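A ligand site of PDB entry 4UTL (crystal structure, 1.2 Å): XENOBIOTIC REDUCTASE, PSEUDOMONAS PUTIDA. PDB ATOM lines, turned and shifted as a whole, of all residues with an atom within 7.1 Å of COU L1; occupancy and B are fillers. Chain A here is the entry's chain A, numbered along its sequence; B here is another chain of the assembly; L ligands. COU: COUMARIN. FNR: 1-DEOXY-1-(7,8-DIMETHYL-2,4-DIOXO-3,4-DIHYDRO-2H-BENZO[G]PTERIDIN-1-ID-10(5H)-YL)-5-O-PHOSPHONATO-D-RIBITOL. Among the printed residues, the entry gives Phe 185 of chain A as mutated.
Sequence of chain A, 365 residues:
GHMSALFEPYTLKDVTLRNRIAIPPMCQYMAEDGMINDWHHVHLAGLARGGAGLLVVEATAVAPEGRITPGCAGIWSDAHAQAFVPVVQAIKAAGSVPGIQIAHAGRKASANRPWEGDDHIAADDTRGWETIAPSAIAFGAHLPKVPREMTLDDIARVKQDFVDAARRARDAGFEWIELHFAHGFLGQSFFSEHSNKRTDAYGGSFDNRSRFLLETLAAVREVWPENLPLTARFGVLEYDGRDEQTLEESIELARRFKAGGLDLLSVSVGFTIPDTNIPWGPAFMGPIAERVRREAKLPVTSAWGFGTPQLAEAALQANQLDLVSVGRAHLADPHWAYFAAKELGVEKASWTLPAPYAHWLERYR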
ATOM      1  N   PRO A  25     -10.797  -3.622   5.939  1.00  0.00           N
ATOM      2  CA  PRO A  25      -9.747  -2.856   5.275  1.00  0.00           C
ATOM      3  C   PRO A  25      -9.378  -3.497   3.932  1.00  0.00           C
ATOM      4  O   PRO A  25      -9.173  -4.703   3.857  1.00  0.00           O
ATOM      5  CB  PRO A  25      -8.587  -2.906   6.290  1.00  0.00           C
ATOM      6  CG  PRO A  25      -8.880  -4.135   7.144  1.00  0.00           C
ATOM      7  CD  PRO A  25     -10.370  -4.173   7.235  1.00  0.00           C
ATOM      8  N   MET A  26      -9.301  -2.675   2.894  1.00  0.00           N
ATOM      9  CA  MET A  26      -8.915  -3.130   1.559  1.00  0.00           C
ATOM     10  C   MET A  26      -8.006  -2.103   0.891  1.00  0.00           C
ATOM     11  O   MET A  26      -8.432  -1.055   0.399  1.00  0.00           O
ATOM     12  CB  MET A  26     -10.106  -3.404   0.654  1.00  0.00           C
ATOM     13  CG  MET A  26     -10.903  -4.636   1.059  1.00  0.00           C
ATOM     14  SD  MET A  26     -12.269  -5.011  -0.046  1.00  0.00           S
ATOM     15  CE  MET A  26     -13.427  -3.722   0.436  1.00  0.00           C
ATOM     16  N   CYS A  27      -6.716  -2.392   0.914  1.00  0.00           N
ATOM     17  CA  CYS A  27      -5.684  -1.620   0.214  1.00  0.00           C
ATOM     18  C   CYS A  27      -6.075  -1.281  -1.191  1.00  0.00           C
ATOM     19  O   CYS A  27      -6.549  -2.150  -1.949  1.00  0.00           O
ATOM     20  CB  CYS A  27      -4.367  -2.410   0.186  1.00  0.00           C
ATOM     21  SG  CYS A  27      -3.443  -2.405   1.719  1.00  0.00           S
ATOM     22  N   TYR A  29      -3.756   0.887  -3.080  1.00  0.00           N
ATOM     23  CA  TYR A  29      -2.471   1.048  -3.780  1.00  0.00           C
ATOM     24  C   TYR A  29      -2.445   2.346  -4.619  1.00  0.00           C
ATOM     25  O   TYR A  29      -1.732   2.415  -5.632  1.00  0.00           O
ATOM     26  CB  TYR A  29      -2.092  -0.175  -4.624  1.00  0.00           C
ATOM     27  CG  TYR A  29      -2.224  -1.479  -3.863  1.00  0.00           C
ATOM     28  CD1 TYR A  29      -1.176  -1.967  -3.085  1.00  0.00           C
ATOM     29  CD2 TYR A  29      -3.410  -2.201  -3.870  1.00  0.00           C
ATOM     30  CE1 TYR A  29      -1.302  -3.142  -2.385  1.00  0.00           C
ATOM     31  CE2 TYR A  29      -3.534  -3.380  -3.161  1.00  0.00           C
ATOM     32  CZ  TYR A  29      -2.481  -3.867  -2.442  1.00  0.00           C
ATOM     33  OH  TYR A  29      -2.632  -5.049  -1.759  1.00  0.00           O
ATOM     34  N   ALA A  59      -5.193  -0.868   5.365  1.00  0.00           N
ATOM     35  CA  ALA A  59      -3.908  -0.865   6.088  1.00  0.00           C
ATOM     36  C   ALA A  59      -3.157   0.426   5.820  1.00  0.00           C
ATOM     37  O   ALA A  59      -2.758   0.692   4.689  1.00  0.00           O
ATOM     38  CB  ALA A  59      -3.076  -2.046   5.639  1.00  0.00           C
ATOM     39  N   ILE A  68       3.231  -1.681   2.564  1.00  0.00           N
ATOM     40  CA  ILE A  68       3.444  -2.854   1.736  1.00  0.00           C
ATOM     41  C   ILE A  68       4.124  -2.429   0.431  1.00  0.00           C
ATOM     42  O   ILE A  68       5.076  -3.085  -0.002  1.00  0.00           O
ATOM     43  CB  ILE A  68       2.144  -3.605   1.434  1.00  0.00           C
ATOM     44  CG1 ILE A  68       1.374  -3.911   2.732  1.00  0.00           C
ATOM     45  CG2 ILE A  68       2.441  -4.868   0.648  1.00  0.00           C
ATOM     46  CD1 ILE A  68      -0.059  -4.314   2.487  1.00  0.00           C
ATOM     47  N   GLN A 101      -7.445   0.822   9.939  1.00  0.00           N
ATOM     48  CA  GLN A 101      -6.469  -0.193  10.286  1.00  0.00           C
ATOM     49  C   GLN A 101      -5.071   0.390  10.209  1.00  0.00           C
ATOM     50  O   GLN A 101      -4.674   0.860   9.147  1.00  0.00           O
ATOM     51  CB  GLN A 101      -6.601  -1.410   9.347  1.00  0.00           C
ATOM     52  CG  GLN A 101      -5.718  -2.566   9.759  1.00  0.00           C
ATOM     53  CD  GLN A 101      -5.708  -3.661   8.728  1.00  0.00           C
ATOM     54  OE1 GLN A 101      -5.311  -3.407   7.604  1.00  0.00           O
ATOM     55  NE2 GLN A 101      -6.113  -4.859   9.094  1.00  0.00           N
ATOM     56  N   PRO A 114      -0.145  -5.254  -6.645  1.00  0.00           N
ATOM     57  CA  PRO A 114      -0.499  -6.619  -7.070  1.00  0.00           C
ATOM     58  C   PRO A 114      -0.645  -6.790  -8.587  1.00  0.00           C
ATOM     59  O   PRO A 114      -0.381  -7.883  -9.097  1.00  0.00           O
ATOM     60  CB  PRO A 114      -1.811  -6.852  -6.345  1.00  0.00           C
ATOM     61  CG  PRO A 114      -1.658  -6.072  -5.055  1.00  0.00           C
ATOM     62  CD  PRO A 114      -1.017  -4.797  -5.532  1.00  0.00           C
ATOM     63  N   ASP A 118       3.430  -7.919  -7.960  1.00  0.00           N
ATOM     64  CA  ASP A 118       3.072  -8.462  -6.644  1.00  0.00           C
ATOM     65  C   ASP A 118       4.268  -8.998  -5.851  1.00  0.00           C
ATOM     66  O   ASP A 118       4.090  -9.628  -4.804  1.00  0.00           O
ATOM     67  CB  ASP A 118       2.007  -9.561  -6.797  1.00  0.00           C
ATOM     68  CG  ASP A 118       1.172  -9.750  -5.548  1.00  0.00           C
ATOM     69  OD1 ASP A 118       0.876  -8.756  -4.850  1.00  0.00           O
ATOM     70  OD2 ASP A 118       0.779 -10.902  -5.258  1.00  0.00           O
ATOM     71  N   HIS A 180      -3.220  -3.952  13.030  1.00  0.00           N
ATOM     72  CA  HIS A 180      -2.993  -5.003  12.054  1.00  0.00           C
ATOM     73  C   HIS A 180      -1.932  -5.987  12.511  1.00  0.00           C
ATOM     74  O   HIS A 180      -0.742  -5.798  12.230  1.00  0.00           O
ATOM     75  CB  HIS A 180      -2.596  -4.423  10.694  1.00  0.00           C
ATOM     76  CG  HIS A 180      -2.764  -5.391   9.579  1.00  0.00           C
ATOM     77  ND1 HIS A 180      -3.022  -6.733   9.790  1.00  0.00           N
ATOM     78  CD2 HIS A 180      -2.792  -5.203   8.237  1.00  0.00           C
ATOM     79  CE1 HIS A 180      -3.207  -7.329   8.617  1.00  0.00           C
ATOM     80  NE2 HIS A 180      -3.063  -6.424   7.661  1.00  0.00           N
ATOM     81  N   ALA A 182      -2.065  -9.251  11.682  1.00  0.00           N
ATOM     82  CA  ALA A 182      -2.337 -10.424  10.873  1.00  0.00           C
ATOM     83  C   ALA A 182      -1.512 -10.453   9.588  1.00  0.00           C
ATOM     84  O   ALA A 182      -0.703  -9.550   9.309  1.00  0.00           O
ATOM     85  CB  ALA A 182      -3.837 -10.508  10.564  1.00  0.00           C
ATOM     86  N   HIS A 183      -1.703 -11.512   8.800  1.00  0.00           N
ATOM     87  CA  HIS A 183      -1.359 -11.564   7.384  1.00  0.00           C
ATOM     88  C   HIS A 183       0.148 -11.551   7.125  1.00  0.00           C
ATOM     89  O   HIS A 183       0.607 -11.202   6.043  1.00  0.00           O
ATOM     90  CB  HIS A 183      -2.091 -10.505   6.571  1.00  0.00           C
ATOM     91  CG  HIS A 183      -3.585 -10.609   6.703  1.00  0.00           C
ATOM     92  ND1 HIS A 183      -4.441  -9.647   6.217  1.00  0.00           N
ATOM     93  CD2 HIS A 183      -4.366 -11.570   7.247  1.00  0.00           C
ATOM     94  CE1 HIS A 183      -5.691  -9.997   6.483  1.00  0.00           C
ATOM     95  NE2 HIS A 183      -5.672 -11.162   7.110  1.00  0.00           N
ATOM     96  N   PHE A 185       2.495  -9.819   8.415  1.00  0.00           N
ATOM     97  CA  PHE A 185       3.128  -8.514   8.579  1.00  0.00           C
ATOM     98  C   PHE A 185       3.838  -8.466   9.934  1.00  0.00           C
ATOM     99  O   PHE A 185       4.064  -9.526  10.578  1.00  0.00           O
ATOM    100  CB  PHE A 185       2.071  -7.430   8.363  1.00  0.00           C
ATOM    101  CG  PHE A 185       1.482  -7.438   6.958  1.00  0.00           C
ATOM    102  CD1 PHE A 185       2.302  -7.514   5.827  1.00  0.00           C
ATOM    103  CD2 PHE A 185       0.115  -7.392   6.773  1.00  0.00           C
ATOM    104  CE1 PHE A 185       1.783  -7.492   4.525  1.00  0.00           C
ATOM    105  CE2 PHE A 185      -0.434  -7.369   5.483  1.00  0.00           C
ATOM    106  CZ  PHE A 185       0.395  -7.428   4.357  1.00  0.00           C
ATOM    107  N   ARG A 233      -6.795  -7.186  14.203  1.00  0.00           N
ATOM    108  CA  ARG A 233      -6.874  -8.324  13.303  1.00  0.00           C
ATOM    109  C   ARG A 233      -5.718  -9.244  13.579  1.00  0.00           C
ATOM    110  O   ARG A 233      -4.581  -8.794  13.714  1.00  0.00           O
ATOM    111  CB  ARG A 233      -6.894  -7.856  11.840  1.00  0.00           C
ATOM    112  CG  ARG A 233      -7.389  -8.946  10.898  1.00  0.00           C
ATOM    113  CD  ARG A 233      -7.710  -8.429   9.512  1.00  0.00           C
ATOM    114  NE  ARG A 233      -8.757  -9.231   8.918  1.00  0.00           N
ATOM    115  CZ  ARG A 233      -9.273  -9.045   7.700  1.00  0.00           C
ATOM    116  NH1 ARG A 233      -8.746  -8.167   6.866  1.00  0.00           N
ATOM    117  NH2 ARG A 233     -10.311  -9.803   7.332  1.00  0.00           N
ATOM    118  N   PHE A 271      -0.975 -16.253   7.110  1.00  0.00           N
ATOM    119  CA  PHE A 271      -0.197 -15.963   5.905  1.00  0.00           C
ATOM    120  C   PHE A 271       1.266 -15.652   6.226  1.00  0.00           C
ATOM    121  O   PHE A 271       1.906 -14.819   5.561  1.00  0.00           O
ATOM    122  CB  PHE A 271      -0.793 -14.809   5.073  1.00  0.00           C
ATOM    123  CG  PHE A 271      -2.237 -15.030   4.680  1.00  0.00           C
ATOM    124  CD1 PHE A 271      -2.568 -15.883   3.644  1.00  0.00           C
ATOM    125  CD2 PHE A 271      -3.256 -14.399   5.359  1.00  0.00           C
ATOM    126  CE1 PHE A 271      -3.891 -16.069   3.269  1.00  0.00           C
ATOM    127  CE2 PHE A 271      -4.583 -14.593   4.982  1.00  0.00           C
ATOM    128  CZ  PHE A 271      -4.893 -15.423   3.947  1.00  0.00           C
ATOM    129  N   TRP A 304     -13.418 -13.581   4.235  1.00  0.00           N
ATOM    130  CA  TRP A 304     -12.875 -14.666   3.415  1.00  0.00           C
ATOM    131  C   TRP A 304     -13.947 -15.647   2.993  1.00  0.00           C
ATOM    132  O   TRP A 304     -13.835 -16.865   3.214  1.00  0.00           O
ATOM    133  CB  TRP A 304     -11.721 -15.409   4.107  1.00  0.00           C
ATOM    134  CG  TRP A 304     -10.644 -14.518   4.649  1.00  0.00           C
ATOM    135  CD1 TRP A 304     -10.439 -14.189   5.961  1.00  0.00           C
ATOM    136  CD2 TRP A 304      -9.599 -13.871   3.910  1.00  0.00           C
ATOM    137  NE1 TRP A 304      -9.341 -13.390   6.082  1.00  0.00           N
ATOM    138  CE2 TRP A 304      -8.797 -13.187   4.844  1.00  0.00           C
ATOM    139  CE3 TRP A 304      -9.236 -13.844   2.557  1.00  0.00           C
ATOM    140  CZ2 TRP A 304      -7.674 -12.450   4.465  1.00  0.00           C
ATOM    141  CZ3 TRP A 304      -8.126 -13.113   2.180  1.00  0.00           C
ATOM    142  CH2 TRP A 304      -7.362 -12.423   3.131  1.00  0.00           C
ATOM    143  N   TRP B 360      -8.862  -7.704  -8.521  1.00  0.00           N
ATOM    144  CA  TRP B 360      -9.385  -8.657  -7.536  1.00  0.00           C
ATOM    145  C   TRP B 360     -10.629  -9.380  -7.975  1.00  0.00           C
ATOM    146  O   TRP B 360     -11.042 -10.320  -7.327  1.00  0.00           O
ATOM    147  CB  TRP B 360      -9.662  -7.918  -6.230  1.00  0.00           C
ATOM    148  CG  TRP B 360      -8.482  -7.143  -5.814  1.00  0.00           C
ATOM    149  CD1 TRP B 360      -8.295  -5.787  -5.923  1.00  0.00           C
ATOM    150  CD2 TRP B 360      -7.250  -7.680  -5.324  1.00  0.00           C
ATOM    151  NE1 TRP B 360      -7.035  -5.465  -5.497  1.00  0.00           N
ATOM    152  CE2 TRP B 360      -6.380  -6.600  -5.095  1.00  0.00           C
ATOM    153  CE3 TRP B 360      -6.805  -8.970  -5.018  1.00  0.00           C
ATOM    154  CZ2 TRP B 360      -5.105  -6.769  -4.595  1.00  0.00           C
ATOM    155  CZ3 TRP B 360      -5.546  -9.148  -4.539  1.00  0.00           C
ATOM    156  CH2 TRP B 360      -4.694  -8.045  -4.316  1.00  0.00           C
HETATM  157  C1  COU L   1      -3.575  -7.321   3.647  1.00  0.00           C
HETATM  158  C2  COU L   1      -3.061  -6.333   2.774  1.00  0.00           C
HETATM  159  C3  COU L   1      -3.274  -6.446   1.401  1.00  0.00           C
HETATM  160  C4  COU L   1      -3.998  -7.542   0.924  1.00  0.00           C
HETATM  161  C5  COU L   1      -4.267  -7.734  -0.429  1.00  0.00           C
HETATM  162  C6  COU L   1      -5.000  -8.840  -0.849  1.00  0.00           C
HETATM  163  C7  COU L   1      -5.478  -9.763   0.062  1.00  0.00           C
HETATM  164  C8  COU L   1      -5.213  -9.588   1.398  1.00  0.00           C
HETATM  165  C9  COU L   1      -4.488  -8.487   1.807  1.00  0.00           C
HETATM  166  O1  COU L   1      -3.465  -7.327   4.832  1.00  0.00           O
HETATM  167  O2  COU L   1      -4.265  -8.381   3.139  1.00  0.00           O
HETATM  168  C9A FNR L   2      -7.655  -7.031   1.276  1.00  0.00           C
HETATM  169  N10 FNR L   2      -7.514  -7.569   2.569  1.00  0.00           N
HETATM  170  CAA FNR L   2      -6.885  -6.774   3.572  1.00  0.00           C
HETATM  171  N1  FNR L   2      -6.854  -7.181   4.814  1.00  0.00           N
HETATM  172  C2  FNR L   2      -6.318  -6.414   5.712  1.00  0.00           C
HETATM  173  O2  FNR L   2      -6.270  -6.787   6.917  1.00  0.00           O
HETATM  174  N3  FNR L   2      -5.873  -5.151   5.371  1.00  0.00           N
HETATM  175  C4  FNR L   2      -5.881  -4.684   4.170  1.00  0.00           C
HETATM  176  O4  FNR L   2      -5.577  -3.522   3.931  1.00  0.00           O
HETATM  177  C4A FNR L   2      -6.269  -5.567   3.142  1.00  0.00           C
HETATM  178  N5  FNR L   2      -6.194  -5.194   1.809  1.00  0.00           N
HETATM  179  C5A FNR L   2      -6.971  -5.881   0.922  1.00  0.00           C
HETATM  180  C6  FNR L   2      -7.142  -5.313  -0.427  1.00  0.00           C
HETATM  181  C7  FNR L   2      -8.052  -5.935  -1.339  1.00  0.00           C
HETATM  182  C7M FNR L   2      -8.352  -5.212  -2.616  1.00  0.00           C
HETATM  183  C8  FNR L   2      -8.702  -7.098  -0.958  1.00  0.00           C
HETATM  184  C8M FNR L   2      -9.608  -7.768  -1.917  1.00  0.00           C
HETATM  185  C9  FNR L   2      -8.511  -7.671   0.277  1.00  0.00           C
HETATM  186  C1' FNR L   2      -8.364  -8.674   3.005  1.00  0.00           C
HETATM  187  C2' FNR L   2      -9.826  -8.288   3.148  1.00  0.00           C
HETATM  188  O2' FNR L   2     -10.003  -7.447   4.301  1.00  0.00           O
HETATM  189  C3' FNR L   2     -10.760  -9.488   3.306  1.00  0.00           C
HETATM  190  O3' FNR L   2     -10.318 -10.270   4.423  1.00  0.00           O
HETATM  191  C4' FNR L   2     -10.796 -10.393   2.077  1.00  0.00           C
HETATM  192  O4' FNR L   2     -11.114  -9.595   0.910  1.00  0.00           O
HETATM  193  C5' FNR L   2     -11.751 -11.588   2.257  1.00  0.00           C
HETATM  194  O5' FNR L   2     -13.118 -11.118   2.380  1.00  0.00           O
HETATM  195  P   FNR L   2     -14.121 -11.294   1.089  1.00  0.00           P
HETATM  196  O1P FNR L   2     -13.429 -10.528  -0.066  1.00  0.00           O
HETATM  197  O2P FNR L   2     -14.266 -12.768   0.792  1.00  0.00           O
HETATM  198  O3P FNR L   2     -15.424 -10.625   1.578  1.00  0.00           O
HETATM  199  C1  COU L   3      -1.548 -10.701   1.862  1.00  0.00           C
HETATM  200  C2  COU L   3      -2.166 -11.580   2.753  1.00  0.00           C
HETATM  201  C3  COU L   3      -3.120 -12.472   2.281  1.00  0.00           C
HETATM  202  C4  COU L   3      -3.443 -12.497   0.930  1.00  0.00           C
HETATM  203  C5  COU L   3      -4.403 -13.398   0.456  1.00  0.00           C
HETATM  204  C6  COU L   3      -4.729 -13.411  -0.888  1.00  0.00           C
HETATM  205  C7  COU L   3      -4.104 -12.527  -1.768  1.00  0.00           C
HETATM  206  C8  COU L   3      -3.149 -11.634  -1.296  1.00  0.00           C
HETATM  207  C9  COU L   3      -2.815 -11.617   0.059  1.00  0.00           C
HETATM  208  O1  COU L   3      -0.656  -9.867   2.285  1.00  0.00           O
HETATM  209  O2  COU L   3      -1.877 -10.738   0.531  1.00  0.00           O
HETATM  210  C1  COU L   4     -10.893 -15.215  -0.498  1.00  0.00           C
HETATM  211  C2  COU L   4     -10.417 -16.012  -1.535  1.00  0.00           C
HETATM  212  C3  COU L   4      -9.557 -15.467  -2.493  1.00  0.00           C
HETATM  213  C4  COU L   4      -9.176 -14.128  -2.393  1.00  0.00           C
HETATM  214  C5  COU L   4      -8.321 -13.562  -3.329  1.00  0.00           C
HETATM  215  C6  COU L   4      -7.958 -12.230  -3.213  1.00  0.00           C
HETATM  216  C7  COU L   4      -8.440 -11.453  -2.172  1.00  0.00           C
HETATM  217  C8  COU L   4      -9.300 -12.027  -1.238  1.00  0.00           C
HETATM  218  C9  COU L   4      -9.671 -13.357  -1.349  1.00  0.00           C
HETATM  219  O1  COU L   4     -11.662 -15.661   0.378  1.00  0.00           O
HETATM  220  O2  COU L   4     -10.512 -13.904  -0.422  1.00  0.00           O
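O of Pro 25 sits at hydrogen-bond distance from O2' of FNR L2 (2.9 Å). The backbone NH (N) of Ala 59 lies within hydrogen-bond range of an oxygen (O4) of FNR L2, at 3.0 Å. A ring nitrogen (ND1) of His 183 is in hydrogen-bond range of an oxygen (O1) of COU L1 (2.9 Å). An oxygen (O5') of FNR L2 is in hydrogen-bond range of the backbone NH (N) of Trp 304, 3.1 Å away. O1 of COU L1 is in hydrogen-bond range of NE2 of His 180 (3.0 Å). O2 of FNR L2 sits at hydrogen-bond distance from NE2 of His 180, at 3.3 Å. The backbone NH (N) of Cys 27 lies close to an oxygen (O4) of FNR L2 (3.4 Å). ND1 of His 183 sits close to O2 of FNR L2 (3.5 Å). The side-chain sulfur (SG) of Cys 27 is in hydrogen-bond range of an oxygen (O4) of FNR L2, 3.3 Å away. N3 of FNR L2 sits at hydrogen-bond distance from OE1 of Gln 101 (2.9 Å). NH1 of Arg 233 sits at hydrogen-bond distance from O2 of FNR L2.
ND1 of His 180 is in hydrogen-bond range of N of Ala 182.
Merely in contact with COU L1: Phe 185, Tyr 29, Trp 360 of chain B, Ile 68 and Trp 304. Hydrophobic or aromatic side chains that line COU L1: Ile 68, His 180, His 183, Phe 185, Trp 304 and Trp 360 of chain B.
O1 of COU L1 lies close to N3 of FNR L2, 3.3 Å away.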
